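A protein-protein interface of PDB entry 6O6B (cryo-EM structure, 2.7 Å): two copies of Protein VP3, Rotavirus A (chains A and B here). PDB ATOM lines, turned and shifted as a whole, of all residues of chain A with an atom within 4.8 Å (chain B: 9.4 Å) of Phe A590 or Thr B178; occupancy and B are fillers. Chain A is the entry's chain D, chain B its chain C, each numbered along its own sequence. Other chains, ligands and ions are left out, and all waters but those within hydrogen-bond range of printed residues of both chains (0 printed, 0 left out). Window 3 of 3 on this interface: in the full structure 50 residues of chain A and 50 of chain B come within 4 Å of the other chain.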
ATOM      1  N   SER A 586     -31.039 -34.108 -30.774  1.00  0.00           N
ATOM      2  CA  SER A 586     -31.021 -32.991 -29.839  1.00  0.00           C
ATOM      3  C   SER A 586     -29.888 -33.103 -28.834  1.00  0.00           C
ATOM      4  O   SER A 586     -29.160 -32.130 -28.611  1.00  0.00           O
ATOM      5  CB  SER A 586     -32.362 -32.885 -29.122  1.00  0.00           C
ATOM      6  OG  SER A 586     -32.614 -34.017 -28.316  1.00  0.00           O
ATOM      7  N   GLY A 587     -29.703 -34.269 -28.238  1.00  0.00           N
ATOM      8  CA  GLY A 587     -28.586 -34.442 -27.343  1.00  0.00           C
ATOM      9  C   GLY A 587     -27.254 -34.463 -28.032  1.00  0.00           C
ATOM     10  O   GLY A 587     -26.249 -34.072 -27.435  1.00  0.00           O
ATOM     11  N   TYR A 588     -27.228 -34.872 -29.295  1.00  0.00           N
ATOM     12  CA  TYR A 588     -26.012 -34.911 -30.088  1.00  0.00           C
ATOM     13  C   TYR A 588     -25.605 -33.534 -30.583  1.00  0.00           C
ATOM     14  O   TYR A 588     -24.451 -33.339 -30.968  1.00  0.00           O
ATOM     15  CB  TYR A 588     -26.199 -35.867 -31.284  1.00  0.00           C
ATOM     16  CG  TYR A 588     -26.317 -37.359 -30.961  1.00  0.00           C
ATOM     17  CD1 TYR A 588     -25.934 -37.858 -29.741  1.00  0.00           C
ATOM     18  CD2 TYR A 588     -26.812 -38.260 -31.891  1.00  0.00           C
ATOM     19  CE1 TYR A 588     -26.029 -39.179 -29.435  1.00  0.00           C
ATOM     20  CE2 TYR A 588     -26.916 -39.605 -31.596  1.00  0.00           C
ATOM     21  CZ  TYR A 588     -26.520 -40.058 -30.355  1.00  0.00           C
ATOM     22  OH  TYR A 588     -26.601 -41.390 -30.003  1.00  0.00           O
ATOM     23  N   ILE A 589     -26.526 -32.568 -30.560  1.00  0.00           N
ATOM     24  CA  ILE A 589     -26.209 -31.206 -30.970  1.00  0.00           C
ATOM     25  C   ILE A 589     -25.829 -30.370 -29.755  1.00  0.00           C
ATOM     26  O   ILE A 589     -24.891 -29.570 -29.807  1.00  0.00           O
ATOM     27  CB  ILE A 589     -27.389 -30.583 -31.740  1.00  0.00           C
ATOM     28  CG1 ILE A 589     -27.619 -31.338 -33.053  1.00  0.00           C
ATOM     29  CG2 ILE A 589     -27.116 -29.123 -32.062  1.00  0.00           C
ATOM     30  CD1 ILE A 589     -28.936 -31.066 -33.759  1.00  0.00           C
ATOM     31  N   PHE A 590     -26.569 -30.525 -28.654  1.00  0.00           N
ATOM     32  CA  PHE A 590     -26.393 -29.634 -27.513  1.00  0.00           C
ATOM     33  C   PHE A 590     -24.996 -29.740 -26.931  1.00  0.00           C
ATOM     34  O   PHE A 590     -24.361 -28.727 -26.622  1.00  0.00           O
ATOM     35  CB  PHE A 590     -27.413 -29.933 -26.421  1.00  0.00           C
ATOM     36  CG  PHE A 590     -27.278 -29.038 -25.236  1.00  0.00           C
ATOM     37  CD1 PHE A 590     -27.787 -27.761 -25.259  1.00  0.00           C
ATOM     38  CD2 PHE A 590     -26.591 -29.454 -24.118  1.00  0.00           C
ATOM     39  CE1 PHE A 590     -27.635 -26.933 -24.174  1.00  0.00           C
ATOM     40  CE2 PHE A 590     -26.436 -28.628 -23.045  1.00  0.00           C
ATOM     41  CZ  PHE A 590     -26.959 -27.370 -23.074  1.00  0.00           C
ATOM     42  N   ARG A 591     -24.511 -30.962 -26.745  1.00  0.00           N
ATOM     43  CA  ARG A 591     -23.284 -31.142 -25.987  1.00  0.00           C
ATOM     44  C   ARG A 591     -22.069 -30.682 -26.776  1.00  0.00           C
ATOM     45  O   ARG A 591     -21.043 -30.328 -26.190  1.00  0.00           O
ATOM     46  CB  ARG A 591     -23.149 -32.594 -25.552  1.00  0.00           C
ATOM     47  CG  ARG A 591     -22.989 -33.607 -26.645  1.00  0.00           C
ATOM     48  CD  ARG A 591     -22.783 -34.974 -26.039  1.00  0.00           C
ATOM     49  NE  ARG A 591     -23.943 -35.412 -25.264  1.00  0.00           N
ATOM     50  CZ  ARG A 591     -24.969 -36.092 -25.762  1.00  0.00           C
ATOM     51  NH1 ARG A 591     -25.025 -36.421 -27.031  1.00  0.00           N
ATOM     52  NH2 ARG A 591     -25.973 -36.441 -24.988  1.00  0.00           N
ATOM     53  N   ASP A 592     -22.163 -30.663 -28.103  1.00  0.00           N
ATOM     54  CA  ASP A 592     -21.076 -30.097 -28.894  1.00  0.00           C
ATOM     55  C   ASP A 592     -21.108 -28.575 -28.871  1.00  0.00           C
ATOM     56  O   ASP A 592     -20.054 -27.931 -28.844  1.00  0.00           O
ATOM     57  CB  ASP A 592     -21.143 -30.615 -30.330  1.00  0.00           C
ATOM     58  CG  ASP A 592     -20.776 -32.084 -30.438  1.00  0.00           C
ATOM     59  OD1 ASP A 592     -19.937 -32.555 -29.641  1.00  0.00           O
ATOM     60  OD2 ASP A 592     -21.333 -32.779 -31.314  1.00  0.00           O
ATOM     61  N   LEU A 593     -22.302 -27.984 -28.881  1.00  0.00           N
ATOM     62  CA  LEU A 593     -22.409 -26.538 -28.758  1.00  0.00           C
ATOM     63  C   LEU A 593     -21.880 -26.069 -27.415  1.00  0.00           C
ATOM     64  O   LEU A 593     -21.200 -25.041 -27.326  1.00  0.00           O
ATOM     65  CB  LEU A 593     -23.857 -26.100 -28.917  1.00  0.00           C
ATOM     66  CG  LEU A 593     -24.583 -26.297 -30.236  1.00  0.00           C
ATOM     67  CD1 LEU A 593     -25.984 -25.904 -30.043  1.00  0.00           C
ATOM     68  CD2 LEU A 593     -24.009 -25.460 -31.321  1.00  0.00           C
ATOM     69  N   SER A 594     -22.195 -26.803 -26.353  1.00  0.00           N
ATOM     70  CA  SER A 594     -21.797 -26.411 -25.013  1.00  0.00           C
ATOM     71  C   SER A 594     -20.347 -26.738 -24.698  1.00  0.00           C
ATOM     72  O   SER A 594     -19.888 -26.405 -23.601  1.00  0.00           O
ATOM     73  CB  SER A 594     -22.702 -27.091 -23.997  1.00  0.00           C
ATOM     74  OG  SER A 594     -22.458 -28.481 -23.975  1.00  0.00           O
ATOM     75  N   TYR A 614     -23.606 -37.618 -18.975  1.00  0.00           N
ATOM     76  CA  TYR A 614     -24.548 -36.551 -19.288  1.00  0.00           C
ATOM     77  C   TYR A 614     -25.974 -36.997 -19.034  1.00  0.00           C
ATOM     78  O   TYR A 614     -26.806 -36.213 -18.586  1.00  0.00           O
ATOM     79  CB  TYR A 614     -24.388 -36.116 -20.735  1.00  0.00           C
ATOM     80  CG  TYR A 614     -25.302 -34.995 -21.117  1.00  0.00           C
ATOM     81  CD1 TYR A 614     -25.035 -33.702 -20.735  1.00  0.00           C
ATOM     82  CD2 TYR A 614     -26.445 -35.237 -21.844  1.00  0.00           C
ATOM     83  CE1 TYR A 614     -25.875 -32.681 -21.078  1.00  0.00           C
ATOM     84  CE2 TYR A 614     -27.288 -34.227 -22.196  1.00  0.00           C
ATOM     85  CZ  TYR A 614     -27.002 -32.950 -21.806  1.00  0.00           C
ATOM     86  OH  TYR A 614     -27.854 -31.942 -22.157  1.00  0.00           O
ATOM     87  N   SER A 661     -21.462 -29.770 -19.826  1.00  0.00           N
ATOM     88  CA  SER A 661     -22.657 -29.605 -20.635  1.00  0.00           C
ATOM     89  C   SER A 661     -23.913 -29.717 -19.788  1.00  0.00           C
ATOM     90  O   SER A 661     -24.930 -29.081 -20.080  1.00  0.00           O
ATOM     91  CB  SER A 661     -22.653 -30.633 -21.751  1.00  0.00           C
ATOM     92  OG  SER A 661     -21.606 -30.355 -22.649  1.00  0.00           O
ATOM     93  N   GLU A 664     -24.488 -26.221 -18.271  1.00  0.00           N
ATOM     94  CA  GLU A 664     -25.160 -25.411 -19.279  1.00  0.00           C
ATOM     95  C   GLU A 664     -26.618 -25.807 -19.435  1.00  0.00           C
ATOM     96  O   GLU A 664     -27.500 -24.946 -19.470  1.00  0.00           O
ATOM     97  CB  GLU A 664     -24.417 -25.570 -20.599  1.00  0.00           C
ATOM     98  CG  GLU A 664     -24.918 -24.717 -21.750  1.00  0.00           C
ATOM     99  CD  GLU A 664     -24.649 -23.239 -21.562  1.00  0.00           C
ATOM    100  OE1 GLU A 664     -23.697 -22.887 -20.838  1.00  0.00           O
ATOM    101  OE2 GLU A 664     -25.382 -22.424 -22.158  1.00  0.00           O
ATOM    102  N   PHE A 665     -26.887 -27.108 -19.519  1.00  0.00           N
ATOM    103  CA  PHE A 665     -28.255 -27.594 -19.645  1.00  0.00           C
ATOM    104  C   PHE A 665     -29.095 -27.157 -18.457  1.00  0.00           C
ATOM    105  O   PHE A 665     -30.244 -26.729 -18.608  1.00  0.00           O
ATOM    106  CB  PHE A 665     -28.245 -29.113 -19.745  1.00  0.00           C
ATOM    107  CG  PHE A 665     -29.600 -29.721 -19.892  1.00  0.00           C
ATOM    108  CD1 PHE A 665     -30.222 -29.762 -21.118  1.00  0.00           C
ATOM    109  CD2 PHE A 665     -30.258 -30.242 -18.798  1.00  0.00           C
ATOM    110  CE1 PHE A 665     -31.465 -30.330 -21.250  1.00  0.00           C
ATOM    111  CE2 PHE A 665     -31.502 -30.802 -18.924  1.00  0.00           C
ATOM    112  CZ  PHE A 665     -32.111 -30.844 -20.146  1.00  0.00           C
ATOM    113  N   LEU A 668     -29.961 -23.127 -18.418  1.00  0.00           N
ATOM    114  CA  LEU A 668     -31.110 -22.686 -19.195  1.00  0.00           C
ATOM    115  C   LEU A 668     -32.407 -23.092 -18.516  1.00  0.00           C
ATOM    116  O   LEU A 668     -33.284 -22.259 -18.275  1.00  0.00           O
ATOM    117  CB  LEU A 668     -31.030 -23.265 -20.601  1.00  0.00           C
ATOM    118  CG  LEU A 668     -30.084 -22.564 -21.580  1.00  0.00           C
ATOM    119  CD1 LEU A 668     -28.636 -22.845 -21.282  1.00  0.00           C
ATOM    120  CD2 LEU A 668     -30.414 -22.990 -22.983  1.00  0.00           C
ATOM    121  N   GLN A 669     -32.526 -24.368 -18.183  1.00  0.00           N
ATOM    122  CA  GLN A 669     -33.582 -24.914 -17.351  1.00  0.00           C
ATOM    123  C   GLN A 669     -33.660 -24.260 -15.981  1.00  0.00           C
ATOM    124  O   GLN A 669     -34.750 -24.211 -15.400  1.00  0.00           O
ATOM    125  CB  GLN A 669     -33.333 -26.413 -17.164  1.00  0.00           C
ATOM    126  CG  GLN A 669     -34.506 -27.362 -16.894  1.00  0.00           C
ATOM    127  CD  GLN A 669     -35.777 -27.042 -17.633  1.00  0.00           C
ATOM    128  OE1 GLN A 669     -35.774 -26.928 -18.851  1.00  0.00           O
ATOM    129  NE2 GLN A 669     -36.869 -26.920 -16.910  1.00  0.00           N
ATOM    130  N   TYR B  97     -29.905 -28.789 -38.821  1.00  0.00           N
ATOM    131  CA  TYR B  97     -28.752 -28.126 -38.241  1.00  0.00           C
ATOM    132  C   TYR B  97     -27.482 -28.944 -38.420  1.00  0.00           C
ATOM    133  O   TYR B  97     -26.389 -28.374 -38.402  1.00  0.00           O
ATOM    134  CB  TYR B  97     -29.003 -27.856 -36.752  1.00  0.00           C
ATOM    135  CG  TYR B  97     -30.032 -26.797 -36.395  1.00  0.00           C
ATOM    136  CD1 TYR B  97     -30.480 -25.869 -37.320  1.00  0.00           C
ATOM    137  CD2 TYR B  97     -30.531 -26.713 -35.106  1.00  0.00           C
ATOM    138  CE1 TYR B  97     -31.396 -24.905 -36.975  1.00  0.00           C
ATOM    139  CE2 TYR B  97     -31.452 -25.752 -34.760  1.00  0.00           C
ATOM    140  CZ  TYR B  97     -31.878 -24.850 -35.703  1.00  0.00           C
ATOM    141  OH  TYR B  97     -32.793 -23.881 -35.383  1.00  0.00           O
ATOM    142  N   THR B  98     -27.601 -30.254 -38.641  1.00  0.00           N
ATOM    143  CA  THR B  98     -26.441 -31.129 -38.682  1.00  0.00           C
ATOM    144  C   THR B  98     -25.515 -30.825 -39.845  1.00  0.00           C
ATOM    145  O   THR B  98     -24.300 -30.758 -39.638  1.00  0.00           O
ATOM    146  CB  THR B  98     -26.881 -32.586 -38.742  1.00  0.00           C
ATOM    147  OG1 THR B  98     -27.669 -32.807 -39.915  1.00  0.00           O
ATOM    148  CG2 THR B  98     -27.674 -32.941 -37.514  1.00  0.00           C
ATOM    149  N   LEU B 170     -26.614 -18.663 -31.048  1.00  0.00           N
ATOM    150  CA  LEU B 170     -26.105 -19.740 -30.211  1.00  0.00           C
ATOM    151  C   LEU B 170     -26.983 -19.947 -28.991  1.00  0.00           C
ATOM    152  O   LEU B 170     -27.125 -21.072 -28.507  1.00  0.00           O
ATOM    153  CB  LEU B 170     -24.674 -19.440 -29.800  1.00  0.00           C
ATOM    154  CG  LEU B 170     -23.950 -20.475 -28.945  1.00  0.00           C
ATOM    155  CD1 LEU B 170     -23.821 -21.755 -29.695  1.00  0.00           C
ATOM    156  CD2 LEU B 170     -22.575 -19.982 -28.534  1.00  0.00           C
ATOM    157  N   ARG B 171     -27.587 -18.880 -28.483  1.00  0.00           N
ATOM    158  CA  ARG B 171     -28.513 -19.021 -27.374  1.00  0.00           C
ATOM    159  C   ARG B 171     -29.778 -19.741 -27.808  1.00  0.00           C
ATOM    160  O   ARG B 171     -30.225 -20.675 -27.137  1.00  0.00           O
ATOM    161  CB  ARG B 171     -28.849 -17.643 -26.817  1.00  0.00           C
ATOM    162  CG  ARG B 171     -29.146 -17.633 -25.343  1.00  0.00           C
ATOM    163  CD  ARG B 171     -29.324 -16.229 -24.795  1.00  0.00           C
ATOM    164  NE  ARG B 171     -30.128 -15.325 -25.622  1.00  0.00           N
ATOM    165  CZ  ARG B 171     -29.804 -14.089 -26.007  1.00  0.00           C
ATOM    166  NH1 ARG B 171     -28.615 -13.553 -25.759  1.00  0.00           N
ATOM    167  NH2 ARG B 171     -30.681 -13.384 -26.709  1.00  0.00           N
ATOM    168  N   LYS B 172     -30.346 -19.353 -28.950  1.00  0.00           N
ATOM    169  CA  LYS B 172     -31.657 -19.864 -29.332  1.00  0.00           C
ATOM    170  C   LYS B 172     -31.567 -21.237 -29.966  1.00  0.00           C
ATOM    171  O   LYS B 172     -32.457 -22.068 -29.766  1.00  0.00           O
ATOM    172  CB  LYS B 172     -32.340 -18.904 -30.294  1.00  0.00           C
ATOM    173  CG  LYS B 172     -32.601 -17.542 -29.743  1.00  0.00           C
ATOM    174  CD  LYS B 172     -33.598 -17.585 -28.627  1.00  0.00           C
ATOM    175  CE  LYS B 172     -34.003 -16.205 -28.212  1.00  0.00           C
ATOM    176  NZ  LYS B 172     -32.871 -15.527 -27.553  1.00  0.00           N
ATOM    177  N   ILE B 173     -30.511 -21.494 -30.732  1.00  0.00           N
ATOM    178  CA  ILE B 173     -30.286 -22.826 -31.282  1.00  0.00           C
ATOM    179  C   ILE B 173     -30.161 -23.837 -30.152  1.00  0.00           C
ATOM    180  O   ILE B 173     -30.483 -25.019 -30.309  1.00  0.00           O
ATOM    181  CB  ILE B 173     -29.044 -22.819 -32.191  1.00  0.00           C
ATOM    182  CG1 ILE B 173     -29.311 -21.917 -33.400  1.00  0.00           C
ATOM    183  CG2 ILE B 173     -28.675 -24.228 -32.647  1.00  0.00           C
ATOM    184  CD1 ILE B 173     -28.102 -21.559 -34.228  1.00  0.00           C
ATOM    185  N   LYS B 174     -29.693 -23.381 -28.994  1.00  0.00           N
ATOM    186  CA  LYS B 174     -29.588 -24.250 -27.837  1.00  0.00           C
ATOM    187  C   LYS B 174     -30.915 -24.369 -27.105  1.00  0.00           C
ATOM    188  O   LYS B 174     -31.120 -25.319 -26.349  1.00  0.00           O
ATOM    189  CB  LYS B 174     -28.509 -23.725 -26.911  1.00  0.00           C
ATOM    190  CG  LYS B 174     -27.145 -23.877 -27.513  1.00  0.00           C
ATOM    191  CD  LYS B 174     -26.077 -23.186 -26.723  1.00  0.00           C
ATOM    192  CE  LYS B 174     -25.761 -23.921 -25.480  1.00  0.00           C
ATOM    193  NZ  LYS B 174     -24.606 -23.246 -24.871  1.00  0.00           N
ATOM    194  N   GLU B 175     -31.826 -23.418 -27.311  1.00  0.00           N
ATOM    195  CA  GLU B 175     -33.138 -23.512 -26.683  1.00  0.00           C
ATOM    196  C   GLU B 175     -33.963 -24.626 -27.314  1.00  0.00           C
ATOM    197  O   GLU B 175     -34.747 -25.299 -26.634  1.00  0.00           O
ATOM    198  CB  GLU B 175     -33.877 -22.177 -26.778  1.00  0.00           C
ATOM    199  CG  GLU B 175     -33.322 -21.090 -25.878  1.00  0.00           C
ATOM    200  CD  GLU B 175     -34.147 -19.817 -25.911  1.00  0.00           C
ATOM    201  OE1 GLU B 175     -35.105 -19.745 -26.705  1.00  0.00           O
ATOM    202  OE2 GLU B 175     -33.836 -18.885 -25.143  1.00  0.00           O
ATOM    203  N   ARG B 176     -33.810 -24.826 -28.622  1.00  0.00           N
ATOM    204  CA  ARG B 176     -34.602 -25.830 -29.320  1.00  0.00           C
ATOM    205  C   ARG B 176     -34.100 -27.229 -29.043  1.00  0.00           C
ATOM    206  O   ARG B 176     -34.897 -28.163 -28.913  1.00  0.00           O
ATOM    207  CB  ARG B 176     -34.570 -25.563 -30.813  1.00  0.00           C
ATOM    208  CG  ARG B 176     -35.285 -24.320 -31.171  1.00  0.00           C
ATOM    209  CD  ARG B 176     -35.244 -24.060 -32.637  1.00  0.00           C
ATOM    210  NE  ARG B 176     -35.968 -22.836 -32.923  1.00  0.00           N
ATOM    211  CZ  ARG B 176     -36.034 -22.250 -34.107  1.00  0.00           C
ATOM    212  NH1 ARG B 176     -35.417 -22.752 -35.164  1.00  0.00           N
ATOM    213  NH2 ARG B 176     -36.731 -21.141 -34.223  1.00  0.00           N
ATOM    214  N   MET B 177     -32.790 -27.387 -28.925  1.00  0.00           N
ATOM    215  CA  MET B 177     -32.187 -28.662 -28.602  1.00  0.00           C
ATOM    216  C   MET B 177     -32.231 -28.948 -27.108  1.00  0.00           C
ATOM    217  O   MET B 177     -31.619 -29.915 -26.654  1.00  0.00           O
ATOM    218  CB  MET B 177     -30.756 -28.669 -29.130  1.00  0.00           C
ATOM    219  CG  MET B 177     -30.667 -28.468 -30.639  1.00  0.00           C
ATOM    220  SD  MET B 177     -31.438 -29.745 -31.651  1.00  0.00           S
ATOM    221  CE  MET B 177     -32.962 -28.982 -32.188  1.00  0.00           C
ATOM    222  N   THR B 178     -32.952 -28.120 -26.347  1.00  0.00           N
ATOM    223  CA  THR B 178     -33.218 -28.295 -24.931  1.00  0.00           C
ATOM    224  C   THR B 178     -34.679 -28.531 -24.637  1.00  0.00           C
ATOM    225  O   THR B 178     -35.004 -29.453 -23.890  1.00  0.00           O
ATOM    226  CB  THR B 178     -32.820 -27.028 -24.146  1.00  0.00           C
ATOM    227  OG1 THR B 178     -31.414 -26.784 -24.309  1.00  0.00           O
ATOM    228  CG2 THR B 178     -33.201 -27.021 -22.692  1.00  0.00           C
ATOM    229  N   THR B 179     -35.557 -27.721 -25.199  1.00  0.00           N
ATOM    230  CA  THR B 179     -36.947 -27.628 -24.810  1.00  0.00           C
ATOM    231  C   THR B 179     -37.827 -28.294 -25.853  1.00  0.00           C
ATOM    232  O   THR B 179     -37.349 -28.835 -26.860  1.00  0.00           O
ATOM    233  CB  THR B 179     -37.340 -26.165 -24.615  1.00  0.00           C
ATOM    234  OG1 THR B 179     -37.206 -25.461 -25.854  1.00  0.00           O
ATOM    235  CG2 THR B 179     -36.461 -25.511 -23.572  1.00  0.00           C
ATOM    236  N   SER B 180     -39.129 -28.230 -25.613  1.00  0.00           N
ATOM    237  CA  SER B 180     -40.063 -28.995 -26.403  1.00  0.00           C
ATOM    238  C   SER B 180     -40.375 -28.289 -27.711  1.00  0.00           C
ATOM    239  O   SER B 180     -40.591 -27.077 -27.763  1.00  0.00           O
ATOM    240  CB  SER B 180     -41.342 -29.225 -25.616  1.00  0.00           C
ATOM    241  OG  SER B 180     -42.047 -28.014 -25.425  1.00  0.00           O
ATOM    242  N   LEU B 181     -40.371 -29.081 -28.770  1.00  0.00           N
ATOM    243  CA  LEU B 181     -40.892 -28.697 -30.066  1.00  0.00           C
ATOM    244  C   LEU B 181     -42.270 -28.063 -29.903  1.00  0.00           C
ATOM    245  O   LEU B 181     -43.202 -28.751 -29.469  1.00  0.00           O
ATOM    246  CB  LEU B 181     -40.983 -29.937 -30.944  1.00  0.00           C
ATOM    247  CG  LEU B 181     -41.259 -29.898 -32.453  1.00  0.00           C
ATOM    248  CD1 LEU B 181     -42.712 -29.649 -32.849  1.00  0.00           C
ATOM    249  CD2 LEU B 181     -40.187 -29.261 -33.372  1.00  0.00           C
ATOM    250  N   PRO B 182     -42.450 -26.766 -30.211  1.00  0.00           N
ATOM    251  CA  PRO B 182     -43.802 -26.176 -30.149  1.00  0.00           C
ATOM    252  C   PRO B 182     -44.608 -26.440 -31.415  1.00  0.00           C
ATOM    253  O   PRO B 182     -44.621 -25.649 -32.359  1.00  0.00           O
ATOM    254  CB  PRO B 182     -43.497 -24.692 -29.948  1.00  0.00           C
ATOM    255  CG  PRO B 182     -42.232 -24.492 -30.650  1.00  0.00           C
ATOM    256  CD  PRO B 182     -41.434 -25.726 -30.454  1.00  0.00           C
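O of Lys B174 lies within hydrogen-bond range of OG1 of Thr B178 (2.5 Å).
The backbone carbonyl oxygen (O) of Phe A590 is in hydrogen-bond range of the side-chain hydroxyl (OG) of Ser A594 (3.3 Å).
OE2 of Glu A664 is in salt-bridge range of NZ of Lys B174 (2.9 Å).
Printed residues of chain B that touch a printed residue of chain A: Lys B174, Met B177 and Thr B178.
Printed residues of chain A that touch a printed residue of chain B: Ser A586, Ile A589, Phe A590, Leu A593 and Glu A664.
Hydrophobic or aromatic side chains of chain A that line the printed part of chain B: Ile A589, Phe A590 and Leu A593.
Among the printed residues, Asp or Glu carboxylates within 4 Å of a Lys or Arg side-chain nitrogen of the other chain: Glu A664 with Lys B174 (2.9 Å).
No position is printed for both chains.
Of the 6 pairs that touch across the chains among the printed residues, none has its exchanged pair printed and touching as well.
Phe A590 touches two residues of chain B.
Printed residues of chain A within 4 Å of Thr B178: Phe A590.
No residue of chain B comes within 4 Å of Gly A587.
Printed residues of chain A within 4 Å of Met B177: Ser A586 and Ile A589.
Printed residues of chain B within 4 Å of Ser A586: Met B177 (3.7 Å).
Leu B181 touches none of the printed residues of chain A.
The nearest residue of chain B that does not touch Phe A590 is Met B177 (4.2 Å).
Met B177 touches Ser A586 (SD to CA, 3.7 Å).
Ile A589 touches Met B177.
CE of Lys B174 touches CE1 of Phe A590 (3.8 Å).
CE1 of Phe A590 touches OG1 of Thr B178 (3.8 Å).
CG of Lys B174 touches CD1 of Leu A593 (3.4 Å).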
